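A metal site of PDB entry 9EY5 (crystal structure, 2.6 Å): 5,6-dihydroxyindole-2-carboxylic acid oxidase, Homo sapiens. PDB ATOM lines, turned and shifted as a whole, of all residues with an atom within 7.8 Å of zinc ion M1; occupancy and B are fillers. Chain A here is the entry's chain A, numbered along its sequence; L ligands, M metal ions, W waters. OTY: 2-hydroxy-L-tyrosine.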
ATOM      1  N   HIS A 168     -10.702 -28.388 -29.037  1.00  0.00           N
ATOM      2  CA  HIS A 168     -10.646 -27.395 -27.961  1.00  0.00           C
ATOM      3  C   HIS A 168     -11.777 -27.600 -26.959  1.00  0.00           C
ATOM      4  O   HIS A 168     -11.568 -27.493 -25.739  1.00  0.00           O
ATOM      5  CB  HIS A 168     -10.679 -26.010 -28.581  1.00  0.00           C
ATOM      6  CG  HIS A 168     -10.397 -24.901 -27.627  1.00  0.00           C
ATOM      7  ND1 HIS A 168     -11.354 -24.377 -26.780  1.00  0.00           N
ATOM      8  CD2 HIS A 168      -9.278 -24.148 -27.442  1.00  0.00           C
ATOM      9  CE1 HIS A 168     -10.831 -23.371 -26.096  1.00  0.00           C
ATOM     10  NE2 HIS A 168      -9.577 -23.219 -26.477  1.00  0.00           N
ATOM     11  N   SER A 171     -11.079 -30.600 -24.705  1.00  0.00           N
ATOM     12  CA  SER A 171     -10.054 -30.377 -23.690  1.00  0.00           C
ATOM     13  C   SER A 171     -10.553 -29.585 -22.475  1.00  0.00           C
ATOM     14  O   SER A 171      -9.898 -29.651 -21.426  1.00  0.00           O
ATOM     15  CB  SER A 171      -8.846 -29.673 -24.308  1.00  0.00           C
ATOM     16  OG  SER A 171      -9.181 -28.362 -24.724  1.00  0.00           O
ATOM     17  N   VAL A 172     -11.674 -28.858 -22.568  1.00  0.00           N
ATOM     18  CA  VAL A 172     -12.162 -28.044 -21.463  1.00  0.00           C
ATOM     19  C   VAL A 172     -13.486 -28.520 -20.875  1.00  0.00           C
ATOM     20  O   VAL A 172     -13.867 -28.022 -19.794  1.00  0.00           O
ATOM     21  CB  VAL A 172     -12.288 -26.552 -21.836  1.00  0.00           C
ATOM     22  CG1 VAL A 172     -11.025 -26.029 -22.478  1.00  0.00           C
ATOM     23  CG2 VAL A 172     -13.553 -26.297 -22.716  1.00  0.00           C
ATOM     24  N   ASP A 188      -9.332 -28.462 -16.608  1.00  0.00           N
ATOM     25  CA  ASP A 188      -9.087 -27.823 -17.889  1.00  0.00           C
ATOM     26  C   ASP A 188      -7.743 -28.324 -18.430  1.00  0.00           C
ATOM     27  O   ASP A 188      -6.685 -27.922 -17.942  1.00  0.00           O
ATOM     28  CB  ASP A 188      -9.111 -26.314 -17.735  1.00  0.00           C
ATOM     29  CG  ASP A 188      -9.200 -25.579 -19.053  1.00  0.00           C
ATOM     30  OD1 ASP A 188      -8.612 -26.100 -20.043  1.00  0.00           O
ATOM     31  OD2 ASP A 188      -9.840 -24.477 -19.093  1.00  0.00           O
ATOM     32  N   SER A 190      -6.206 -27.638 -21.115  1.00  0.00           N
ATOM     33  CA  SER A 190      -5.483 -26.770 -22.030  1.00  0.00           C
ATOM     34  C   SER A 190      -5.378 -25.326 -21.561  1.00  0.00           C
ATOM     35  O   SER A 190      -4.847 -24.499 -22.314  1.00  0.00           O
ATOM     36  CB  SER A 190      -6.132 -26.806 -23.410  1.00  0.00           C
ATOM     37  OG  SER A 190      -7.548 -26.738 -23.308  1.00  0.00           O
ATOM     38  N   HIS A 191      -5.860 -24.994 -20.362  1.00  0.00           N
ATOM     39  CA  HIS A 191      -5.706 -23.674 -19.776  1.00  0.00           C
ATOM     40  C   HIS A 191      -5.431 -23.825 -18.300  1.00  0.00           C
ATOM     41  O   HIS A 191      -5.604 -24.906 -17.723  1.00  0.00           O
ATOM     42  CB  HIS A 191      -6.945 -22.809 -19.966  1.00  0.00           C
ATOM     43  CG  HIS A 191      -7.560 -22.964 -21.320  1.00  0.00           C
ATOM     44  ND1 HIS A 191      -8.316 -24.054 -21.674  1.00  0.00           N
ATOM     45  CD2 HIS A 191      -7.463 -22.189 -22.425  1.00  0.00           C
ATOM     46  CE1 HIS A 191      -8.691 -23.934 -22.931  1.00  0.00           C
ATOM     47  NE2 HIS A 191      -8.201 -22.805 -23.408  1.00  0.00           N
ATOM     48  N   PHE A 196      -0.933 -24.883 -21.194  1.00  0.00           N
ATOM     49  CA  PHE A 196      -1.703 -23.938 -21.997  1.00  0.00           C
ATOM     50  C   PHE A 196      -0.968 -23.523 -23.269  1.00  0.00           C
ATOM     51  O   PHE A 196      -1.533 -23.582 -24.372  1.00  0.00           O
ATOM     52  CB  PHE A 196      -2.046 -22.692 -21.158  1.00  0.00           C
ATOM     53  CG  PHE A 196      -2.412 -21.486 -21.986  1.00  0.00           C
ATOM     54  CD1 PHE A 196      -3.675 -21.392 -22.578  1.00  0.00           C
ATOM     55  CD2 PHE A 196      -1.505 -20.453 -22.183  1.00  0.00           C
ATOM     56  CE1 PHE A 196      -4.009 -20.279 -23.341  1.00  0.00           C
ATOM     57  CE2 PHE A 196      -1.846 -19.333 -22.944  1.00  0.00           C
ATOM     58  CZ  PHE A 196      -3.096 -19.256 -23.531  1.00  0.00           C
ATOM     59  N   TRP A 199      -0.178 -26.709 -25.651  1.00  0.00           N
ATOM     60  CA  TRP A 199      -1.397 -27.281 -26.204  1.00  0.00           C
ATOM     61  C   TRP A 199      -1.867 -26.442 -27.386  1.00  0.00           C
ATOM     62  O   TRP A 199      -2.121 -26.963 -28.479  1.00  0.00           O
ATOM     63  CB  TRP A 199      -2.474 -27.378 -25.125  1.00  0.00           C
ATOM     64  CG  TRP A 199      -3.716 -28.164 -25.538  1.00  0.00           C
ATOM     65  CD1 TRP A 199      -4.024 -29.437 -25.169  1.00  0.00           C
ATOM     66  CD2 TRP A 199      -4.793 -27.718 -26.380  1.00  0.00           C
ATOM     67  NE1 TRP A 199      -5.230 -29.826 -25.724  1.00  0.00           N
ATOM     68  CE2 TRP A 199      -5.714 -28.788 -26.474  1.00  0.00           C
ATOM     69  CE3 TRP A 199      -5.065 -26.524 -27.053  1.00  0.00           C
ATOM     70  CZ2 TRP A 199      -6.887 -28.691 -27.229  1.00  0.00           C
ATOM     71  CZ3 TRP A 199      -6.231 -26.437 -27.801  1.00  0.00           C
ATOM     72  CH2 TRP A 199      -7.123 -27.513 -27.878  1.00  0.00           C
ATOM     73  N   HIS A 200      -1.951 -25.132 -27.188  1.00  0.00           N
ATOM     74  CA  HIS A 200      -2.414 -24.247 -28.244  1.00  0.00           C
ATOM     75  C   HIS A 200      -1.414 -24.142 -29.387  1.00  0.00           C
ATOM     76  O   HIS A 200      -1.821 -23.988 -30.548  1.00  0.00           O
ATOM     77  CB  HIS A 200      -2.699 -22.867 -27.665  1.00  0.00           C
ATOM     78  CG  HIS A 200      -3.948 -22.812 -26.861  1.00  0.00           C
ATOM     79  ND1 HIS A 200      -3.988 -23.087 -25.506  1.00  0.00           N
ATOM     80  CD2 HIS A 200      -5.216 -22.494 -27.222  1.00  0.00           C
ATOM     81  CE1 HIS A 200      -5.227 -22.944 -25.075  1.00  0.00           C
ATOM     82  NE2 HIS A 200      -5.991 -22.593 -26.098  1.00  0.00           N
ATOM     83  N   HIS A 203      -2.215 -27.109 -31.399  1.00  0.00           N
ATOM     84  CA  HIS A 203      -3.532 -26.823 -31.953  1.00  0.00           C
ATOM     85  C   HIS A 203      -3.408 -26.070 -33.275  1.00  0.00           C
ATOM     86  O   HIS A 203      -3.978 -26.474 -34.296  1.00  0.00           O
ATOM     87  CB  HIS A 203      -4.326 -26.012 -30.926  1.00  0.00           C
ATOM     88  CG  HIS A 203      -5.799 -25.987 -31.163  1.00  0.00           C
ATOM     89  ND1 HIS A 203      -6.569 -24.891 -30.861  1.00  0.00           N
ATOM     90  CD2 HIS A 203      -6.648 -26.933 -31.646  1.00  0.00           C
ATOM     91  CE1 HIS A 203      -7.837 -25.152 -31.145  1.00  0.00           C
ATOM     92  NE2 HIS A 203      -7.907 -26.388 -31.632  1.00  0.00           N
ATOM     93  N   GLU A 336      -0.805 -16.002 -20.496  1.00  0.00           N
ATOM     94  CA  GLU A 336      -2.182 -16.475 -20.517  1.00  0.00           C
ATOM     95  C   GLU A 336      -3.142 -15.375 -20.051  1.00  0.00           C
ATOM     96  O   GLU A 336      -4.222 -15.204 -20.616  1.00  0.00           O
ATOM     97  CB  GLU A 336      -2.340 -17.731 -19.657  1.00  0.00           C
ATOM     98  CG  GLU A 336      -3.739 -18.361 -19.772  1.00  0.00           C
ATOM     99  CD  GLU A 336      -3.848 -19.717 -19.091  1.00  0.00           C
ATOM    100  OE1 GLU A 336      -2.879 -20.118 -18.413  1.00  0.00           O
ATOM    101  OE2 GLU A 336      -4.895 -20.392 -19.229  1.00  0.00           O
ATOM    102  N   HIS A 353      -3.513 -12.480 -23.281  1.00  0.00           N
ATOM    103  CA  HIS A 353      -4.345 -13.447 -24.011  1.00  0.00           C
ATOM    104  C   HIS A 353      -5.763 -13.488 -23.459  1.00  0.00           C
ATOM    105  O   HIS A 353      -6.730 -13.529 -24.240  1.00  0.00           O
ATOM    106  CB  HIS A 353      -3.721 -14.852 -23.960  1.00  0.00           C
ATOM    107  CG  HIS A 353      -4.723 -15.981 -23.980  1.00  0.00           C
ATOM    108  ND1 HIS A 353      -5.401 -16.390 -22.846  1.00  0.00           N
ATOM    109  CD2 HIS A 353      -5.162 -16.781 -24.978  1.00  0.00           C
ATOM    110  CE1 HIS A 353      -6.205 -17.388 -23.149  1.00  0.00           C
ATOM    111  NE2 HIS A 353      -6.070 -17.649 -24.422  1.00  0.00           N
ATOM    112  N   ASN A 354      -5.925 -13.497 -22.134  1.00  0.00           N
ATOM    113  CA  ASN A 354      -7.277 -13.512 -21.560  1.00  0.00           C
ATOM    114  C   ASN A 354      -7.997 -12.214 -21.841  1.00  0.00           C
ATOM    115  O   ASN A 354      -9.189 -12.216 -22.174  1.00  0.00           O
ATOM    116  CB  ASN A 354      -7.236 -13.754 -20.047  1.00  0.00           C
ATOM    117  CG  ASN A 354      -7.018 -15.209 -19.693  1.00  0.00           C
ATOM    118  OD1 ASN A 354      -7.306 -16.110 -20.493  1.00  0.00           O
ATOM    119  ND2 ASN A 354      -6.503 -15.447 -18.492  1.00  0.00           N
ATOM    120  N   HIS A 357      -9.397 -12.151 -25.462  1.00  0.00           N
ATOM    121  CA  HIS A 357     -10.645 -12.888 -25.600  1.00  0.00           C
ATOM    122  C   HIS A 357     -11.847 -12.083 -25.101  1.00  0.00           C
ATOM    123  O   HIS A 357     -12.856 -11.955 -25.789  1.00  0.00           O
ATOM    124  CB  HIS A 357     -10.559 -14.193 -24.827  1.00  0.00           C
ATOM    125  CG  HIS A 357      -9.940 -15.310 -25.581  1.00  0.00           C
ATOM    126  ND1 HIS A 357     -10.680 -16.189 -26.357  1.00  0.00           N
ATOM    127  CD2 HIS A 357      -8.668 -15.739 -25.647  1.00  0.00           C
ATOM    128  CE1 HIS A 357      -9.875 -17.088 -26.878  1.00  0.00           C
ATOM    129  NE2 HIS A 357      -8.646 -16.834 -26.478  1.00  0.00           N
ATOM    130  N   GLN A 366     -16.309 -17.231 -24.734  1.00  0.00           N
ATOM    131  CA  GLN A 366     -16.769 -18.396 -23.998  1.00  0.00           C
ATOM    132  C   GLN A 366     -15.783 -19.561 -24.183  1.00  0.00           C
ATOM    133  O   GLN A 366     -15.497 -19.973 -25.314  1.00  0.00           O
ATOM    134  CB  GLN A 366     -18.166 -18.748 -24.484  1.00  0.00           C
ATOM    135  CG  GLN A 366     -18.933 -17.473 -24.861  1.00  0.00           C
ATOM    136  CD  GLN A 366     -20.397 -17.711 -25.132  1.00  0.00           C
ATOM    137  OE1 GLN A 366     -20.875 -17.468 -26.252  1.00  0.00           O
ATOM    138  NE2 GLN A 366     -21.111 -18.194 -24.120  1.00  0.00           N
ATOM    139  N   THR A 367     -15.266 -20.106 -23.068  1.00  0.00           N
ATOM    140  CA  THR A 367     -14.121 -21.008 -23.172  1.00  0.00           C
ATOM    141  C   THR A 367     -14.458 -22.265 -23.975  1.00  0.00           C
ATOM    142  O   THR A 367     -13.587 -22.775 -24.695  1.00  0.00           O
ATOM    143  CB  THR A 367     -13.593 -21.387 -21.783  1.00  0.00           C
ATOM    144  OG1 THR A 367     -13.265 -20.198 -21.051  1.00  0.00           O
ATOM    145  CG2 THR A 367     -12.316 -22.312 -21.915  1.00  0.00           C
ATOM    146  N   SER A 370     -14.942 -20.630 -27.966  1.00  0.00           N
ATOM    147  CA  SER A 370     -14.186 -19.523 -28.556  1.00  0.00           C
ATOM    148  C   SER A 370     -13.585 -19.791 -29.935  1.00  0.00           C
ATOM    149  O   SER A 370     -13.627 -18.876 -30.769  1.00  0.00           O
ATOM    150  CB  SER A 370     -13.092 -19.068 -27.576  1.00  0.00           C
ATOM    151  OG  SER A 370     -12.470 -20.187 -26.987  1.00  0.00           O
ATOM    152  N   PRO A 371     -13.032 -20.973 -30.253  1.00  0.00           N
ATOM    153  CA  PRO A 371     -12.476 -21.162 -31.616  1.00  0.00           C
ATOM    154  C   PRO A 371     -13.499 -21.001 -32.742  1.00  0.00           C
ATOM    155  O   PRO A 371     -13.079 -20.948 -33.911  1.00  0.00           O
ATOM    156  CB  PRO A 371     -11.912 -22.589 -31.577  1.00  0.00           C
ATOM    157  CG  PRO A 371     -11.784 -22.930 -30.152  1.00  0.00           C
ATOM    158  CD  PRO A 371     -12.838 -22.181 -29.431  1.00  0.00           C
ATOM    159  N   PHE A 376      -9.975 -16.335 -33.225  1.00  0.00           N
ATOM    160  CA  PHE A 376      -9.266 -17.256 -32.337  1.00  0.00           C
ATOM    161  C   PHE A 376      -7.916 -17.633 -32.927  1.00  0.00           C
ATOM    162  O   PHE A 376      -6.880 -17.559 -32.258  1.00  0.00           O
ATOM    163  CB  PHE A 376     -10.104 -18.512 -32.094  1.00  0.00           C
ATOM    164  CG  PHE A 376      -9.494 -19.476 -31.105  1.00  0.00           C
ATOM    165  CD1 PHE A 376      -8.420 -20.283 -31.458  1.00  0.00           C
ATOM    166  CD2 PHE A 376      -9.987 -19.561 -29.803  1.00  0.00           C
ATOM    167  CE1 PHE A 376      -7.834 -21.161 -30.536  1.00  0.00           C
ATOM    168  CE2 PHE A 376      -9.415 -20.441 -28.871  1.00  0.00           C
ATOM    169  CZ  PHE A 376      -8.342 -21.243 -29.243  1.00  0.00           C
ATOM    170  N   HIS A 380      -4.236 -16.556 -31.324  1.00  0.00           N
ATOM    171  CA  HIS A 380      -3.336 -17.556 -30.777  1.00  0.00           C
ATOM    172  C   HIS A 380      -2.025 -17.665 -31.508  1.00  0.00           C
ATOM    173  O   HIS A 380      -1.006 -17.963 -30.868  1.00  0.00           O
ATOM    174  CB  HIS A 380      -4.019 -18.910 -30.722  1.00  0.00           C
ATOM    175  CG  HIS A 380      -4.796 -19.044 -29.471  1.00  0.00           C
ATOM    176  ND1 HIS A 380      -4.198 -19.377 -28.262  1.00  0.00           N
ATOM    177  CD2 HIS A 380      -6.071 -18.713 -29.182  1.00  0.00           C
ATOM    178  CE1 HIS A 380      -5.105 -19.324 -27.312  1.00  0.00           C
ATOM    179  NE2 HIS A 380      -6.239 -18.928 -27.852  1.00  0.00           N
HETATM  180  OD1 OTY L   1     -12.719 -15.873 -22.262  1.00  0.00           O
HETATM  181  N   OTY L   1     -10.857 -15.362 -18.051  1.00  0.00           N
HETATM  182  CA  OTY L   1     -11.406 -15.900 -19.311  1.00  0.00           C
HETATM  183  C   OTY L   1     -11.872 -17.357 -19.115  1.00  0.00           C
HETATM  184  O   OTY L   1     -12.984 -17.730 -19.591  1.00  0.00           O
HETATM  185  CB  OTY L   1     -10.344 -15.798 -20.481  1.00  0.00           C
HETATM  186  CG  OTY L   1     -10.536 -16.856 -21.616  1.00  0.00           C
HETATM  187  CD1 OTY L   1     -11.669 -16.854 -22.432  1.00  0.00           C
HETATM  188  CD2 OTY L   1      -9.537 -17.855 -21.870  1.00  0.00           C
HETATM  189  CE1 OTY L   1     -11.842 -17.826 -23.482  1.00  0.00           C
HETATM  190  CE2 OTY L   1      -9.686 -18.845 -22.885  1.00  0.00           C
HETATM  191  CZ  OTY L   1     -10.852 -18.808 -23.688  1.00  0.00           C
HETATM  192  OH  OTY L   1     -11.063 -19.779 -24.756  1.00  0.00           O
HETATM  193  OXT OTY L   1     -11.150 -18.202 -18.478  1.00  0.00           O
HETATM  194 ZN    ZN M   1      -7.993 -22.011 -25.486  1.00  0.00          ZN
HETATM  195 ZN    ZN M   2      -7.328 -18.577 -25.968  1.00  0.00          ZN
HETATM  196  O   HOH W   1      -8.435 -20.033 -25.632  1.00  0.00           O
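The side-chain hydroxyl (OG) of Ser 370 sits at hydrogen-bond distance from an oxygen (OH) of the ligand, 2.7 Å away. The side-chain hydroxyl (OG1) of Thr 367 is in hydrogen-bond range of an oxygen (O) of the ligand (2.9 Å).
ND1 of His 200 is in hydrogen-bond range of O of Phe 196 (2.7 Å). A ring nitrogen (ND1) of His 168 lies close to the backbone carbonyl oxygen of Thr 367. The backbone carbonyl oxygen (O) of His 168 lies within hydrogen-bond range of the side-chain hydroxyl (OG) of Ser 171 (2.7 Å). ND1 of His 191 sits close to OG of Ser 190. The side-chain carboxylate (OD1) of Asp 188 sits at hydrogen-bond distance from a ring nitrogen (ND1) of His 191 (2.6 Å).
Residues that only touch zinc ion M1: Phe 376 (3.9 Å). Within 4 Å of zinc ion M1: His 168, His 191, His 200 and Phe 376. Along chain A the residues within 4 Å of zinc ion M1 span positions 168 to 376.
Zinc ion M1 is bound by water W1 (2.0 Å). A ring nitrogen (NE2) of His 200 binds zinc ion M1 (2.2 Å). NE2 of His 168 is bound to zinc ion M1 (2.2 Å). NE2 of His 191 is bound to zinc ion M1, at 2.2 Å. Zinc ion M1 has four donor atoms within binding distance.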
